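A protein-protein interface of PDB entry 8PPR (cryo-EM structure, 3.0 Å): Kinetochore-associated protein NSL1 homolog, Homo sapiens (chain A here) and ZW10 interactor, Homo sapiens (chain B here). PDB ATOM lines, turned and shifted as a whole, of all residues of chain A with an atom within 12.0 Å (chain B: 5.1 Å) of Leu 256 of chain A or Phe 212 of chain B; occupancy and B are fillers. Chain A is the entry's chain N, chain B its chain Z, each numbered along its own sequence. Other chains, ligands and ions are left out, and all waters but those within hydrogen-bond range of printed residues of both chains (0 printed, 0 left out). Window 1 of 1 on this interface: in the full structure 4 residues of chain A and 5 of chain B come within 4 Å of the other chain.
Printed residues of chain A that touch a printed residue of chain B: Met 254, Leu 256, Lys 257 and Arg 258. Hydrophobic or aromatic side chains of chain A that line the printed part of chain B: Met 254 and Leu 256. Hydrophobic or aromatic side chains of chain B within 4 Å of the printed part of chain A: Phe 212, Leu 215 and Leu 216. Among the printed residues, 7 pairs touch across the chains.
Met 254 of chain A touches Thr 211 of chain B. Met 254 of chain A touches Leu 215 of chain B (CE to CG, 3.5 Å). Leu 256 of chain A touches Phe 212 of chain B. Leu 256 of chain A touches Leu 216 of chain B (CD1 to CD1, 3.9 Å). Phe 212 of chain B touches Lys 257 of chain A (CE1 to N, 3.6 Å). Arg 258 of chain A touches Phe 212 of chain B.
Of the printed residues of chain B, Met 254 of chain A touches Arg 208, Thr 211 and Leu 215. Leu 256 of chain A touches just these residues of chain B: Phe 212 (3.3 Å) and Leu 216 (3.9 Å). Of the printed residues of chain B, Lys 257 of chain A touches Phe 212. Printed residues of chain B within 4 Å of Arg 258 of chain A: Phe 212. Gln 207 of chain B touches none of the printed residues of chain A. Of chain A, only Met 254 comes within 4 Å of Arg 208 of chain B. Tyr 209 of chain B touches none of the printed residues of chain A. Of chain A, only Met 254 comes within 4 Å of Thr 211 of chain B. No residue of chain A comes within 4 Å of Leu 213 of chain B. Leu 215 of chain B touches just one residue of chain A: Met 254. Leu 216 of chain B touches one residue of chain A. The nearest residue of chain B that does not touch Leu 256 of chain A is Leu 215 of chain B (4.1 Å). The nearest printed residue of chain B that does not touch Arg 258 of chain A is Leu 216 of chain B (5.5 Å).
The side-chain amide nitrogen of Gln 214 of chain B sits at hydrogen-bond distance from the side-chain hydroxyl of Thr 211 of chain B (2.9 Å).
The side-chain sulfur (SD) of Met 254 of chain A sits close to the guanidinium group (NH2) of Arg 208 of chain B (3.8 Å).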
ATOM      1  N   THR A 251      -3.823  20.496 -31.622  1.00  0.00           N
ATOM      2  CA  THR A 251      -4.338  21.855 -31.708  1.00  0.00           C
ATOM      3  C   THR A 251      -4.038  22.620 -30.425  1.00  0.00           C
ATOM      4  O   THR A 251      -3.976  22.043 -29.336  1.00  0.00           O
ATOM      5  CB  THR A 251      -5.845  21.837 -31.969  1.00  0.00           C
ATOM      6  OG1 THR A 251      -6.512  21.182 -30.882  1.00  0.00           O
ATOM      7  CG2 THR A 251      -6.150  21.094 -33.261  1.00  0.00           C
ATOM      8  N   SER A 252      -3.849  23.932 -30.561  1.00  0.00           N
ATOM      9  CA  SER A 252      -3.592  24.779 -29.405  1.00  0.00           C
ATOM     10  C   SER A 252      -4.881  24.966 -28.619  1.00  0.00           C
ATOM     11  O   SER A 252      -5.606  25.944 -28.823  1.00  0.00           O
ATOM     12  CB  SER A 252      -3.029  26.133 -29.838  1.00  0.00           C
ATOM     13  OG  SER A 252      -3.991  26.872 -30.571  1.00  0.00           O
ATOM     14  N   ASP A 253      -5.176  24.031 -27.723  1.00  0.00           N
ATOM     15  CA  ASP A 253      -6.424  24.031 -26.972  1.00  0.00           C
ATOM     16  C   ASP A 253      -6.184  24.387 -25.505  1.00  0.00           C
ATOM     17  O   ASP A 253      -5.529  23.646 -24.766  1.00  0.00           O
ATOM     18  CB  ASP A 253      -7.155  22.693 -27.145  1.00  0.00           C
ATOM     19  CG  ASP A 253      -6.371  21.485 -26.622  1.00  0.00           C
ATOM     20  OD1 ASP A 253      -5.224  21.622 -26.155  1.00  0.00           O
ATOM     21  OD2 ASP A 253      -6.926  20.368 -26.678  1.00  0.00           O
ATOM     22  N   MET A 254      -6.693  25.545 -25.092  1.00  0.00           N
ATOM     23  CA  MET A 254      -6.845  25.819 -23.669  1.00  0.00           C
ATOM     24  C   MET A 254      -8.103  25.090 -23.235  1.00  0.00           C
ATOM     25  O   MET A 254      -9.220  25.502 -23.545  1.00  0.00           O
ATOM     26  CB  MET A 254      -6.918  27.313 -23.377  1.00  0.00           C
ATOM     27  CG  MET A 254      -7.020  27.588 -21.883  1.00  0.00           C
ATOM     28  SD  MET A 254      -7.086  29.315 -21.380  1.00  0.00           S
ATOM     29  CE  MET A 254      -8.727  29.754 -21.900  1.00  0.00           C
ATOM     30  N   VAL A 255      -7.908  23.969 -22.536  1.00  0.00           N
ATOM     31  CA  VAL A 255      -9.039  23.129 -22.155  1.00  0.00           C
ATOM     32  C   VAL A 255     -10.063  23.944 -21.375  1.00  0.00           C
ATOM     33  O   VAL A 255     -11.273  23.842 -21.615  1.00  0.00           O
ATOM     34  CB  VAL A 255      -8.554  21.895 -21.367  1.00  0.00           C
ATOM     35  CG1 VAL A 255      -7.635  21.041 -22.236  1.00  0.00           C
ATOM     36  CG2 VAL A 255      -7.858  22.289 -20.064  1.00  0.00           C
ATOM     37  N   LEU A 256      -9.590  24.792 -20.457  1.00  0.00           N
ATOM     38  CA  LEU A 256     -10.453  25.668 -19.665  1.00  0.00           C
ATOM     39  C   LEU A 256     -11.533  24.849 -18.963  1.00  0.00           C
ATOM     40  O   LEU A 256     -12.685  25.268 -18.835  1.00  0.00           O
ATOM     41  CB  LEU A 256     -11.061  26.772 -20.541  1.00  0.00           C
ATOM     42  CG  LEU A 256     -11.635  28.038 -19.896  1.00  0.00           C
ATOM     43  CD1 LEU A 256     -10.615  28.683 -18.991  1.00  0.00           C
ATOM     44  CD2 LEU A 256     -12.079  29.039 -20.938  1.00  0.00           C
ATOM     45  N   LYS A 257     -11.151  23.658 -18.506  1.00  0.00           N
ATOM     46  CA  LYS A 257     -12.074  22.707 -17.900  1.00  0.00           C
ATOM     47  C   LYS A 257     -11.913  22.746 -16.387  1.00  0.00           C
ATOM     48  O   LYS A 257     -10.809  22.543 -15.869  1.00  0.00           O
ATOM     49  CB  LYS A 257     -11.831  21.292 -18.427  1.00  0.00           C
ATOM     50  CG  LYS A 257     -11.727  21.199 -19.938  1.00  0.00           C
ATOM     51  CD  LYS A 257     -11.580  19.761 -20.411  1.00  0.00           C
ATOM     52  CE  LYS A 257     -12.832  18.955 -20.116  1.00  0.00           C
ATOM     53  NZ  LYS A 257     -14.031  19.570 -20.752  1.00  0.00           N
ATOM     54  N   ARG A 258     -13.009  23.016 -15.688  1.00  0.00           N
ATOM     55  CA  ARG A 258     -13.025  23.035 -14.236  1.00  0.00           C
ATOM     56  C   ARG A 258     -13.407  21.652 -13.706  1.00  0.00           C
ATOM     57  O   ARG A 258     -13.489  20.674 -14.455  1.00  0.00           O
ATOM     58  CB  ARG A 258     -13.960  24.142 -13.747  1.00  0.00           C
ATOM     59  CG  ARG A 258     -15.427  23.940 -14.092  1.00  0.00           C
ATOM     60  CD  ARG A 258     -16.249  25.129 -13.615  1.00  0.00           C
ATOM     61  NE  ARG A 258     -17.669  24.996 -13.915  1.00  0.00           N
ATOM     62  CZ  ARG A 258     -18.590  25.893 -13.585  1.00  0.00           C
ATOM     63  NH1 ARG A 258     -18.273  27.001 -12.933  1.00  0.00           N
ATOM     64  NH2 ARG A 258     -19.858  25.675 -13.918  1.00  0.00           N
ATOM     65  N   LYS A 259     -13.640  21.557 -12.402  1.00  0.00           N
ATOM     66  CA  LYS A 259     -13.930  20.305 -11.722  1.00  0.00           C
ATOM     67  C   LYS A 259     -15.407  20.243 -11.327  1.00  0.00           C
ATOM     68  O   LYS A 259     -16.206  21.117 -11.683  1.00  0.00           O
ATOM     69  CB  LYS A 259     -12.979  20.145 -10.528  1.00  0.00           C
ATOM     70  CG  LYS A 259     -13.124  21.190  -9.420  1.00  0.00           C
ATOM     71  CD  LYS A 259     -14.120  20.789  -8.342  1.00  0.00           C
ATOM     72  CE  LYS A 259     -14.145  21.810  -7.216  1.00  0.00           C
ATOM     73  NZ  LYS A 259     -15.129  21.448  -6.161  1.00  0.00           N
ATOM     74  N   GLN A 260     -15.768  19.181 -10.600  1.00  0.00           N
ATOM     75  CA  GLN A 260     -17.130  18.945 -10.119  1.00  0.00           C
ATOM     76  C   GLN A 260     -18.095  18.748 -11.294  1.00  0.00           C
ATOM     77  O   GLN A 260     -19.036  19.514 -11.514  1.00  0.00           O
ATOM     78  CB  GLN A 260     -17.588  20.076  -9.184  1.00  0.00           C
ATOM     79  CG  GLN A 260     -18.972  19.891  -8.561  1.00  0.00           C
ATOM     80  CD  GLN A 260     -19.057  18.663  -7.676  1.00  0.00           C
ATOM     81  OE1 GLN A 260     -19.638  17.648  -8.059  1.00  0.00           O
ATOM     82  NE2 GLN A 260     -18.479  18.751  -6.484  1.00  0.00           N
ATOM     83  N   THR A 261     -17.816  17.708 -12.074  1.00  0.00           N
ATOM     84  CA  THR A 261     -18.695  17.261 -13.148  1.00  0.00           C
ATOM     85  C   THR A 261     -19.234  15.883 -12.784  1.00  0.00           C
ATOM     86  O   THR A 261     -18.455  14.943 -12.588  1.00  0.00           O
ATOM     87  CB  THR A 261     -17.958  17.219 -14.486  1.00  0.00           C
ATOM     88  OG1 THR A 261     -16.837  16.331 -14.388  1.00  0.00           O
ATOM     89  CG2 THR A 261     -17.467  18.609 -14.866  1.00  0.00           C
ATOM     90  N   GLN B 207       1.229  28.281 -15.417  1.00  0.00           N
ATOM     91  CA  GLN B 207       0.544  29.156 -16.360  1.00  0.00           C
ATOM     92  C   GLN B 207      -0.813  28.592 -16.741  1.00  0.00           C
ATOM     93  O   GLN B 207      -1.728  29.355 -17.070  1.00  0.00           O
ATOM     94  CB  GLN B 207       1.407  29.378 -17.604  1.00  0.00           C
ATOM     95  CG  GLN B 207       1.853  28.104 -18.310  1.00  0.00           C
ATOM     96  CD  GLN B 207       0.825  27.576 -19.294  1.00  0.00           C
ATOM     97  OE1 GLN B 207       0.086  28.345 -19.908  1.00  0.00           O
ATOM     98  NE2 GLN B 207       0.773  26.258 -19.446  1.00  0.00           N
ATOM     99  N   ARG B 208      -0.964  27.267 -16.662  1.00  0.00           N
ATOM    100  CA  ARG B 208      -2.250  26.640 -16.933  1.00  0.00           C
ATOM    101  C   ARG B 208      -3.339  27.263 -16.073  1.00  0.00           C
ATOM    102  O   ARG B 208      -4.252  27.927 -16.581  1.00  0.00           O
ATOM    103  CB  ARG B 208      -2.174  25.138 -16.647  1.00  0.00           C
ATOM    104  CG  ARG B 208      -3.490  24.418 -16.889  1.00  0.00           C
ATOM    105  CD  ARG B 208      -3.676  24.244 -18.387  1.00  0.00           C
ATOM    106  NE  ARG B 208      -4.106  25.465 -19.054  1.00  0.00           N
ATOM    107  CZ  ARG B 208      -4.027  25.661 -20.361  1.00  0.00           C
ATOM    108  NH1 ARG B 208      -3.659  24.694 -21.184  1.00  0.00           N
ATOM    109  NH2 ARG B 208      -4.284  26.868 -20.850  1.00  0.00           N
ATOM    110  N   TYR B 209      -3.233  27.084 -14.754  1.00  0.00           N
ATOM    111  CA  TYR B 209      -4.253  27.588 -13.844  1.00  0.00           C
ATOM    112  C   TYR B 209      -4.258  29.107 -13.795  1.00  0.00           C
ATOM    113  O   TYR B 209      -5.303  29.712 -13.543  1.00  0.00           O
ATOM    114  CB  TYR B 209      -4.055  27.006 -12.445  1.00  0.00           C
ATOM    115  CG  TYR B 209      -4.332  25.525 -12.358  1.00  0.00           C
ATOM    116  CD1 TYR B 209      -5.008  24.865 -13.376  1.00  0.00           C
ATOM    117  CD2 TYR B 209      -3.933  24.788 -11.252  1.00  0.00           C
ATOM    118  CE1 TYR B 209      -5.268  23.512 -13.300  1.00  0.00           C
ATOM    119  CE2 TYR B 209      -4.190  23.434 -11.167  1.00  0.00           C
ATOM    120  CZ  TYR B 209      -4.858  22.802 -12.193  1.00  0.00           C
ATOM    121  OH  TYR B 209      -5.116  21.453 -12.113  1.00  0.00           O
ATOM    122  N   GLN B 210      -3.112  29.750 -14.036  1.00  0.00           N
ATOM    123  CA  GLN B 210      -3.101  31.210 -14.027  1.00  0.00           C
ATOM    124  C   GLN B 210      -3.982  31.778 -15.140  1.00  0.00           C
ATOM    125  O   GLN B 210      -4.872  32.605 -14.887  1.00  0.00           O
ATOM    126  CB  GLN B 210      -1.669  31.728 -14.145  1.00  0.00           C
ATOM    127  CG  GLN B 210      -0.855  31.528 -12.880  1.00  0.00           C
ATOM    128  CD  GLN B 210       0.520  32.154 -12.963  1.00  0.00           C
ATOM    129  OE1 GLN B 210       1.342  31.769 -13.794  1.00  0.00           O
ATOM    130  NE2 GLN B 210       0.775  33.132 -12.103  1.00  0.00           N
ATOM    131  N   THR B 211      -3.769  31.324 -16.380  1.00  0.00           N
ATOM    132  CA  THR B 211      -4.591  31.824 -17.477  1.00  0.00           C
ATOM    133  C   THR B 211      -6.022  31.315 -17.358  1.00  0.00           C
ATOM    134  O   THR B 211      -6.966  32.023 -17.718  1.00  0.00           O
ATOM    135  CB  THR B 211      -3.976  31.452 -18.831  1.00  0.00           C
ATOM    136  OG1 THR B 211      -4.666  32.150 -19.876  1.00  0.00           O
ATOM    137  CG2 THR B 211      -4.070  29.952 -19.097  1.00  0.00           C
ATOM    138  N   PHE B 212      -6.200  30.102 -16.832  1.00  0.00           N
ATOM    139  CA  PHE B 212      -7.532  29.592 -16.532  1.00  0.00           C
ATOM    140  C   PHE B 212      -8.296  30.558 -15.628  1.00  0.00           C
ATOM    141  O   PHE B 212      -9.393  31.021 -15.967  1.00  0.00           O
ATOM    142  CB  PHE B 212      -7.366  28.216 -15.877  1.00  0.00           C
ATOM    143  CG  PHE B 212      -8.642  27.525 -15.532  1.00  0.00           C
ATOM    144  CD1 PHE B 212      -9.417  26.921 -16.499  1.00  0.00           C
ATOM    145  CD2 PHE B 212      -9.048  27.437 -14.217  1.00  0.00           C
ATOM    146  CE1 PHE B 212     -10.590  26.273 -16.164  1.00  0.00           C
ATOM    147  CE2 PHE B 212     -10.207  26.794 -13.886  1.00  0.00           C
ATOM    148  CZ  PHE B 212     -10.980  26.210 -14.851  1.00  0.00           C
ATOM    149  N   LEU B 213      -7.686  30.925 -14.500  1.00  0.00           N
ATOM    150  CA  LEU B 213      -8.339  31.798 -13.535  1.00  0.00           C
ATOM    151  C   LEU B 213      -8.600  33.176 -14.117  1.00  0.00           C
ATOM    152  O   LEU B 213      -9.655  33.767 -13.866  1.00  0.00           O
ATOM    153  CB  LEU B 213      -7.487  31.901 -12.273  1.00  0.00           C
ATOM    154  CG  LEU B 213      -8.081  32.703 -11.113  1.00  0.00           C
ATOM    155  CD1 LEU B 213      -9.385  32.076 -10.646  1.00  0.00           C
ATOM    156  CD2 LEU B 213      -7.089  32.801  -9.968  1.00  0.00           C
ATOM    157  N   GLN B 214      -7.656  33.718 -14.889  1.00  0.00           N
ATOM    158  CA  GLN B 214      -7.899  35.066 -15.392  1.00  0.00           C
ATOM    159  C   GLN B 214      -8.901  35.086 -16.547  1.00  0.00           C
ATOM    160  O   GLN B 214      -9.604  36.088 -16.723  1.00  0.00           O
ATOM    161  CB  GLN B 214      -6.574  35.758 -15.740  1.00  0.00           C
ATOM    162  CG  GLN B 214      -5.668  35.135 -16.788  1.00  0.00           C
ATOM    163  CD  GLN B 214      -5.942  35.621 -18.195  1.00  0.00           C
ATOM    164  OE1 GLN B 214      -6.476  36.712 -18.396  1.00  0.00           O
ATOM    165  NE2 GLN B 214      -5.482  34.860 -19.177  1.00  0.00           N
ATOM    166  N   LEU B 215      -9.036  33.997 -17.315  1.00  0.00           N
ATOM    167  CA  LEU B 215     -10.193  33.903 -18.205  1.00  0.00           C
ATOM    168  C   LEU B 215     -11.501  33.833 -17.432  1.00  0.00           C
ATOM    169  O   LEU B 215     -12.487  34.454 -17.836  1.00  0.00           O
ATOM    170  CB  LEU B 215     -10.090  32.729 -19.180  1.00  0.00           C
ATOM    171  CG  LEU B 215      -9.305  32.913 -20.483  1.00  0.00           C
ATOM    172  CD1 LEU B 215     -10.011  33.972 -21.321  1.00  0.00           C
ATOM    173  CD2 LEU B 215      -7.868  33.285 -20.300  1.00  0.00           C
ATOM    174  N   LEU B 216     -11.555  33.071 -16.338  1.00  0.00           N
ATOM    175  CA  LEU B 216     -12.787  33.117 -15.548  1.00  0.00           C
ATOM    176  C   LEU B 216     -13.051  34.520 -15.003  1.00  0.00           C
ATOM    177  O   LEU B 216     -14.208  34.948 -14.920  1.00  0.00           O
ATOM    178  CB  LEU B 216     -12.782  32.080 -14.423  1.00  0.00           C
ATOM    179  CG  LEU B 216     -13.090  30.609 -14.752  1.00  0.00           C
ATOM    180  CD1 LEU B 216     -12.020  29.859 -15.514  1.00  0.00           C
ATOM    181  CD2 LEU B 216     -13.431  29.877 -13.466  1.00  0.00           C
